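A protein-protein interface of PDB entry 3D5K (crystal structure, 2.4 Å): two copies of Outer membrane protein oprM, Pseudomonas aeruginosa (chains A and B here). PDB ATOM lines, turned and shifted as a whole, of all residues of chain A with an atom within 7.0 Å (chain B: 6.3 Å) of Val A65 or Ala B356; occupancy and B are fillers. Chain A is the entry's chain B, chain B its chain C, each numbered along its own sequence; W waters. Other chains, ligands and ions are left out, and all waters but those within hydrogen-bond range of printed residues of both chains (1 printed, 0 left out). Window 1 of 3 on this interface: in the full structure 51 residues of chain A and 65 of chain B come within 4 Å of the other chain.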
ATOM      1  N   ASN A  60      16.353 -23.533  -8.812  1.00  0.00           N
ATOM      2  CA  ASN A  60      16.145 -23.347 -10.254  1.00  0.00           C
ATOM      3  C   ASN A  60      14.745 -23.767 -10.697  1.00  0.00           C
ATOM      4  O   ASN A  60      14.319 -24.896 -10.453  1.00  0.00           O
ATOM      5  CB  ASN A  60      17.224 -24.066 -11.068  1.00  0.00           C
ATOM      6  CG  ASN A  60      17.088 -23.837 -12.564  1.00  0.00           C
ATOM      7  OD1 ASN A  60      16.233 -24.420 -13.215  1.00  0.00           O
ATOM      8  ND2 ASN A  60      17.945 -22.993 -13.113  1.00  0.00           N
ATOM      9  N   ARG A  61      14.045 -22.848 -11.355  1.00  0.00           N
ATOM     10  CA  ARG A  61      12.636 -23.045 -11.699  1.00  0.00           C
ATOM     11  C   ARG A  61      12.383 -24.046 -12.829  1.00  0.00           C
ATOM     12  O   ARG A  61      11.329 -24.689 -12.852  1.00  0.00           O
ATOM     13  CB  ARG A  61      11.942 -21.705 -11.993  1.00  0.00           C
ATOM     14  CG  ARG A  61      11.913 -20.700 -10.830  1.00  0.00           C
ATOM     15  CD  ARG A  61      11.697 -21.374  -9.480  1.00  0.00           C
ATOM     16  NE  ARG A  61      11.184 -20.460  -8.465  1.00  0.00           N
ATOM     17  CZ  ARG A  61      11.915 -19.895  -7.509  1.00  0.00           C
ATOM     18  NH1 ARG A  61      13.213 -20.135  -7.416  1.00  0.00           N
ATOM     19  NH2 ARG A  61      11.337 -19.082  -6.638  1.00  0.00           N
ATOM     20  N   ASP A  62      13.343 -24.184 -13.749  1.00  0.00           N
ATOM     21  CA  ASP A  62      13.246 -25.165 -14.839  1.00  0.00           C
ATOM     22  C   ASP A  62      13.239 -26.589 -14.308  1.00  0.00           C
ATOM     23  O   ASP A  62      12.437 -27.414 -14.741  1.00  0.00           O
ATOM     24  CB  ASP A  62      14.404 -25.018 -15.830  1.00  0.00           C
ATOM     25  CG  ASP A  62      14.262 -23.808 -16.728  1.00  0.00           C
ATOM     26  OD1 ASP A  62      13.138 -23.543 -17.216  1.00  0.00           O
ATOM     27  OD2 ASP A  62      15.291 -23.132 -16.962  1.00  0.00           O
ATOM     28  N   LEU A  63      14.150 -26.868 -13.378  1.00  0.00           N
ATOM     29  CA  LEU A  63      14.240 -28.174 -12.742  1.00  0.00           C
ATOM     30  C   LEU A  63      13.031 -28.429 -11.851  1.00  0.00           C
ATOM     31  O   LEU A  63      12.586 -29.568 -11.713  1.00  0.00           O
ATOM     32  CB  LEU A  63      15.539 -28.296 -11.934  1.00  0.00           C
ATOM     33  CG  LEU A  63      15.848 -29.647 -11.263  1.00  0.00           C
ATOM     34  CD1 LEU A  63      15.840 -30.797 -12.272  1.00  0.00           C
ATOM     35  CD2 LEU A  63      17.168 -29.604 -10.494  1.00  0.00           C
ATOM     36  N   ARG A  64      12.501 -27.362 -11.256  1.00  0.00           N
ATOM     37  CA  ARG A  64      11.316 -27.452 -10.412  1.00  0.00           C
ATOM     38  C   ARG A  64      10.093 -27.876 -11.232  1.00  0.00           C
ATOM     39  O   ARG A  64       9.353 -28.769 -10.819  1.00  0.00           O
ATOM     40  CB  ARG A  64      11.078 -26.127  -9.678  1.00  0.00           C
ATOM     41  CG  ARG A  64      10.285 -26.248  -8.386  1.00  0.00           C
ATOM     42  CD  ARG A  64      10.205 -24.909  -7.640  1.00  0.00           C
ATOM     43  NE  ARG A  64      11.292 -24.749  -6.675  1.00  0.00           N
ATOM     44  CZ  ARG A  64      11.374 -23.772  -5.772  1.00  0.00           C
ATOM     45  NH1 ARG A  64      10.438 -22.832  -5.695  1.00  0.00           N
ATOM     46  NH2 ARG A  64      12.405 -23.734  -4.940  1.00  0.00           N
ATOM     47  N   VAL A  65       9.902 -27.253 -12.399  1.00  0.00           N
ATOM     48  CA  VAL A  65       8.842 -27.642 -13.347  1.00  0.00           C
ATOM     49  C   VAL A  65       9.014 -29.092 -13.818  1.00  0.00           C
ATOM     50  O   VAL A  65       8.033 -29.818 -13.992  1.00  0.00           O
ATOM     51  CB  VAL A  65       8.782 -26.692 -14.579  1.00  0.00           C
ATOM     52  CG1 VAL A  65       7.793 -27.201 -15.628  1.00  0.00           C
ATOM     53  CG2 VAL A  65       8.419 -25.267 -14.155  1.00  0.00           C
ATOM     54  N   ALA A  66      10.262 -29.506 -14.019  1.00  0.00           N
ATOM     55  CA  ALA A  66      10.570 -30.883 -14.388  1.00  0.00           C
ATOM     56  C   ALA A  66      10.171 -31.877 -13.288  1.00  0.00           C
ATOM     57  O   ALA A  66       9.646 -32.958 -13.585  1.00  0.00           O
ATOM     58  CB  ALA A  66      12.047 -31.026 -14.742  1.00  0.00           C
ATOM     59  N   ALA A  67      10.404 -31.501 -12.028  1.00  0.00           N
ATOM     60  CA  ALA A  67      10.016 -32.323 -10.873  1.00  0.00           C
ATOM     61  C   ALA A  67       8.502 -32.468 -10.751  1.00  0.00           C
ATOM     62  O   ALA A  67       7.996 -33.473 -10.234  1.00  0.00           O
ATOM     63  CB  ALA A  67      10.592 -31.742  -9.586  1.00  0.00           C
ATOM     64  N   LEU A  68       7.786 -31.458 -11.240  1.00  0.00           N
ATOM     65  CA  LEU A  68       6.337 -31.415 -11.147  1.00  0.00           C
ATOM     66  C   LEU A  68       5.654 -32.172 -12.284  1.00  0.00           C
ATOM     67  O   LEU A  68       4.605 -32.780 -12.078  1.00  0.00           O
ATOM     68  CB  LEU A  68       5.851 -29.959 -11.071  1.00  0.00           C
ATOM     69  CG  LEU A  68       6.090 -29.196  -9.756  1.00  0.00           C
ATOM     70  CD1 LEU A  68       6.026 -27.688  -9.973  1.00  0.00           C
ATOM     71  CD2 LEU A  68       5.101 -29.625  -8.670  1.00  0.00           C
ATOM     72  N   ASN A  69       6.245 -32.135 -13.479  1.00  0.00           N
ATOM     73  CA  ASN A  69       5.761 -32.941 -14.609  1.00  0.00           C
ATOM     74  C   ASN A  69       5.670 -34.436 -14.264  1.00  0.00           C
ATOM     75  O   ASN A  69       4.718 -35.109 -14.660  1.00  0.00           O
ATOM     76  CB  ASN A  69       6.640 -32.752 -15.852  1.00  0.00           C
ATOM     77  CG  ASN A  69       6.429 -31.408 -16.543  1.00  0.00           C
ATOM     78  OD1 ASN A  69       7.337 -30.898 -17.205  1.00  0.00           O
ATOM     79  ND2 ASN A  69       5.238 -30.841 -16.411  1.00  0.00           N
ATOM     80  N   VAL A  70       6.661 -34.939 -13.521  1.00  0.00           N
ATOM     81  CA  VAL A  70       6.669 -36.322 -13.023  1.00  0.00           C
ATOM     82  C   VAL A  70       5.403 -36.612 -12.225  1.00  0.00           C
ATOM     83  O   VAL A  70       4.759 -37.642 -12.434  1.00  0.00           O
ATOM     84  CB  VAL A  70       7.907 -36.618 -12.138  1.00  0.00           C
ATOM     85  CG1 VAL A  70       7.917 -38.076 -11.683  1.00  0.00           C
ATOM     86  CG2 VAL A  70       9.192 -36.290 -12.875  1.00  0.00           C
ATOM     87  N   LYS B 351      -1.115 -25.791 -11.239  1.00  0.00           N
ATOM     88  CA  LYS B 351      -1.012 -24.470 -10.624  1.00  0.00           C
ATOM     89  C   LYS B 351       0.415 -24.181 -10.167  1.00  0.00           C
ATOM     90  O   LYS B 351       0.915 -23.070 -10.359  1.00  0.00           O
ATOM     91  CB  LYS B 351      -1.981 -24.317  -9.450  1.00  0.00           C
ATOM     92  CG  LYS B 351      -2.071 -22.878  -8.926  1.00  0.00           C
ATOM     93  CD  LYS B 351      -2.731 -22.804  -7.570  1.00  0.00           C
ATOM     94  CE  LYS B 351      -2.850 -21.365  -7.111  1.00  0.00           C
ATOM     95  NZ  LYS B 351      -3.806 -21.225  -5.967  1.00  0.00           N
ATOM     96  N   ASP B 352       1.062 -25.178  -9.565  1.00  0.00           N
ATOM     97  CA  ASP B 352       2.437 -25.034  -9.080  1.00  0.00           C
ATOM     98  C   ASP B 352       3.476 -24.924 -10.198  1.00  0.00           C
ATOM     99  O   ASP B 352       4.526 -24.301 -10.016  1.00  0.00           O
ATOM    100  CB  ASP B 352       2.798 -26.184  -8.139  1.00  0.00           C
ATOM    101  CG  ASP B 352       2.035 -26.128  -6.832  1.00  0.00           C
ATOM    102  OD1 ASP B 352       1.568 -25.027  -6.444  1.00  0.00           O
ATOM    103  OD2 ASP B 352       1.907 -27.195  -6.191  1.00  0.00           O
ATOM    104  N   ILE B 353       3.188 -25.551 -11.337  1.00  0.00           N
ATOM    105  CA  ILE B 353       4.001 -25.407 -12.540  1.00  0.00           C
ATOM    106  C   ILE B 353       3.922 -23.952 -12.998  1.00  0.00           C
ATOM    107  O   ILE B 353       4.938 -23.342 -13.339  1.00  0.00           O
ATOM    108  CB  ILE B 353       3.534 -26.371 -13.658  1.00  0.00           C
ATOM    109  CG1 ILE B 353       4.003 -27.799 -13.357  1.00  0.00           C
ATOM    110  CG2 ILE B 353       4.037 -25.919 -15.034  1.00  0.00           C
ATOM    111  CD1 ILE B 353       3.228 -28.899 -14.081  1.00  0.00           C
ATOM    112  N   ASN B 354       2.712 -23.398 -12.965  1.00  0.00           N
ATOM    113  CA  ASN B 354       2.483 -22.001 -13.325  1.00  0.00           C
ATOM    114  C   ASN B 354       3.056 -21.002 -12.327  1.00  0.00           C
ATOM    115  O   ASN B 354       3.438 -19.900 -12.713  1.00  0.00           O
ATOM    116  CB  ASN B 354       1.000 -21.737 -13.579  1.00  0.00           C
ATOM    117  CG  ASN B 354       0.556 -22.207 -14.956  1.00  0.00           C
ATOM    118  OD1 ASN B 354       0.942 -21.638 -15.978  1.00  0.00           O
ATOM    119  ND2 ASN B 354      -0.257 -23.249 -14.987  1.00  0.00           N
ATOM    120  N   VAL B 355       3.133 -21.387 -11.055  1.00  0.00           N
ATOM    121  CA  VAL B 355       3.821 -20.565 -10.063  1.00  0.00           C
ATOM    122  C   VAL B 355       5.291 -20.440 -10.463  1.00  0.00           C
ATOM    123  O   VAL B 355       5.808 -19.325 -10.600  1.00  0.00           O
ATOM    124  CB  VAL B 355       3.686 -21.130  -8.624  1.00  0.00           C
ATOM    125  CG1 VAL B 355       4.599 -20.386  -7.661  1.00  0.00           C
ATOM    126  CG2 VAL B 355       2.249 -21.033  -8.147  1.00  0.00           C
ATOM    127  N   ALA B 356       5.936 -21.588 -10.674  1.00  0.00           N
ATOM    128  CA  ALA B 356       7.345 -21.658 -11.057  1.00  0.00           C
ATOM    129  C   ALA B 356       7.641 -20.951 -12.381  1.00  0.00           C
ATOM    130  O   ALA B 356       8.649 -20.263 -12.504  1.00  0.00           O
ATOM    131  CB  ALA B 356       7.802 -23.110 -11.117  1.00  0.00           C
ATOM    132  N   GLN B 357       6.765 -21.129 -13.364  1.00  0.00           N
ATOM    133  CA  GLN B 357       6.925 -20.492 -14.672  1.00  0.00           C
ATOM    134  C   GLN B 357       6.815 -18.969 -14.576  1.00  0.00           C
ATOM    135  O   GLN B 357       7.571 -18.235 -15.217  1.00  0.00           O
ATOM    136  CB  GLN B 357       5.910 -21.054 -15.667  1.00  0.00           C
ATOM    137  CG  GLN B 357       6.271 -22.445 -16.191  1.00  0.00           C
ATOM    138  CD  GLN B 357       5.150 -23.101 -16.985  1.00  0.00           C
ATOM    139  OE1 GLN B 357       3.968 -22.830 -16.764  1.00  0.00           O
ATOM    140  NE2 GLN B 357       5.521 -23.986 -17.905  1.00  0.00           N
ATOM    141  N   TYR B 358       5.886 -18.505 -13.747  1.00  0.00           N
ATOM    142  CA  TYR B 358       5.712 -17.077 -13.491  1.00  0.00           C
ATOM    143  C   TYR B 358       6.933 -16.491 -12.776  1.00  0.00           C
ATOM    144  O   TYR B 358       7.345 -15.365 -13.056  1.00  0.00           O
ATOM    145  CB  TYR B 358       4.420 -16.841 -12.696  1.00  0.00           C
ATOM    146  CG  TYR B 358       4.284 -15.467 -12.096  1.00  0.00           C
ATOM    147  CD1 TYR B 358       4.057 -14.351 -12.902  1.00  0.00           C
ATOM    148  CD2 TYR B 358       4.372 -15.283 -10.717  1.00  0.00           C
ATOM    149  CE1 TYR B 358       3.935 -13.088 -12.350  1.00  0.00           C
ATOM    150  CE2 TYR B 358       4.248 -14.026 -10.154  1.00  0.00           C
ATOM    151  CZ  TYR B 358       4.031 -12.935 -10.972  1.00  0.00           C
ATOM    152  OH  TYR B 358       3.911 -11.689 -10.412  1.00  0.00           O
ATOM    153  N   GLU B 359       7.518 -17.268 -11.868  1.00  0.00           N
ATOM    154  CA  GLU B 359       8.711 -16.851 -11.136  1.00  0.00           C
ATOM    155  C   GLU B 359       9.951 -16.800 -12.031  1.00  0.00           C
ATOM    156  O   GLU B 359      10.743 -15.861 -11.953  1.00  0.00           O
ATOM    157  CB  GLU B 359       8.952 -17.781  -9.947  1.00  0.00           C
ATOM    158  CG  GLU B 359       8.013 -17.555  -8.770  1.00  0.00           C
ATOM    159  CD  GLU B 359       8.165 -18.620  -7.696  1.00  0.00           C
ATOM    160  OE1 GLU B 359       8.470 -19.782  -8.043  1.00  0.00           O
ATOM    161  OE2 GLU B 359       7.975 -18.293  -6.501  1.00  0.00           O
ATOM    162  N   LYS B 360      10.115 -17.818 -12.869  1.00  0.00           N
ATOM    163  CA  LYS B 360      11.203 -17.862 -13.844  1.00  0.00           C
ATOM    164  C   LYS B 360      11.097 -16.674 -14.805  1.00  0.00           C
ATOM    165  O   LYS B 360      12.111 -16.095 -15.199  1.00  0.00           O
ATOM    166  CB  LYS B 360      11.188 -19.188 -14.611  1.00  0.00           C
ATOM    167  CG  LYS B 360      12.266 -19.325 -15.685  1.00  0.00           C
ATOM    168  CD  LYS B 360      11.757 -20.212 -16.812  1.00  0.00           C
ATOM    169  CE  LYS B 360      12.611 -20.110 -18.071  1.00  0.00           C
ATOM    170  NZ  LYS B 360      11.844 -20.579 -19.266  1.00  0.00           N
ATOM    171  N   ALA B 361       9.865 -16.316 -15.158  1.00  0.00           N
ATOM    172  CA  ALA B 361       9.582 -15.133 -15.974  1.00  0.00           C
ATOM    173  C   ALA B 361      10.125 -13.856 -15.340  1.00  0.00           C
ATOM    174  O   ALA B 361      10.675 -13.003 -16.037  1.00  0.00           O
ATOM    175  CB  ALA B 361       8.088 -15.004 -16.239  1.00  0.00           C
HETATM  176  O   HOH W   1       7.948 -22.309  -7.314  1.00  0.00           O
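Water W1 lies within hydrogen-bond range of OE1 of Glu B359 (2.7 Å) and NH1 of Arg A64 (3.0 Å).
The side-chain amide oxygen of Asn A60 sits at hydrogen-bond distance from the backbone NH of Asp A62.
The side-chain amide oxygen (OD1) of Asn A69 lies close to the backbone carbonyl oxygen (O) of Val A65, at 3.5 Å.
No position is printed for both chains.
Of the 8 pairs that touch across the chains among the printed residues, none has its exchanged pair printed and touching as well.
Printed residues of chain B within 4 Å of Val A65: Ala B356.
Ala B356 touches just these residues of chain A: Arg A61 (3.6 Å) and Val A65 (3.8 Å).
Of the printed residues of chain A, Lys B360 touches Arg A61 and Asp A62.
Of the printed residues of chain B, Arg A61 touches Ala B356 (3.6 Å), Glu B359 (2.8 Å) and Lys B360 (3.7 Å).
Of the printed residues of chain A, Asp B352 touches Leu A68 (3.7 Å).
Printed residues of chain B within 4 Å of Asn A69: Ile B353 (3.6 Å).
Val A70 touches none of the printed residues of chain B.
The nearest residue of chain A that does not touch Ala B356 is Arg A64 (4.6 Å).
The nearest printed residue of chain A that does not touch Asp B352 is Val A65 (5.8 Å).
Ala B356 touches Arg A61 (O to CB, 3.6 Å).
CB of Lys B360 touches CB of Arg A61 (3.7 Å).
Val A65 touches Ala B356 (CG2 to CB, 3.8 Å).
CD1 of Leu A68 touches O of Asp B352, 3.7 Å away.
CB of Leu A68 touches CG1 of Ile B353 (3.6 Å).
CD1 of Ile B353 touches ND2 of Asn A69 (3.6 Å).
Hydrophobic or aromatic side chains of chain A that line the printed part of chain B: Val A65 and Leu A68.
Along chain B the printed residues that touch a printed residue of chain A span positions 352 to 360.
The guanidinium group of Arg A61 is in salt-bridge range of the side-chain carboxylate of Glu B359, at 2.8 Å.
OD1 of Asp A62 is in salt-bridge range of NZ of Lys B360, at 3.8 Å.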
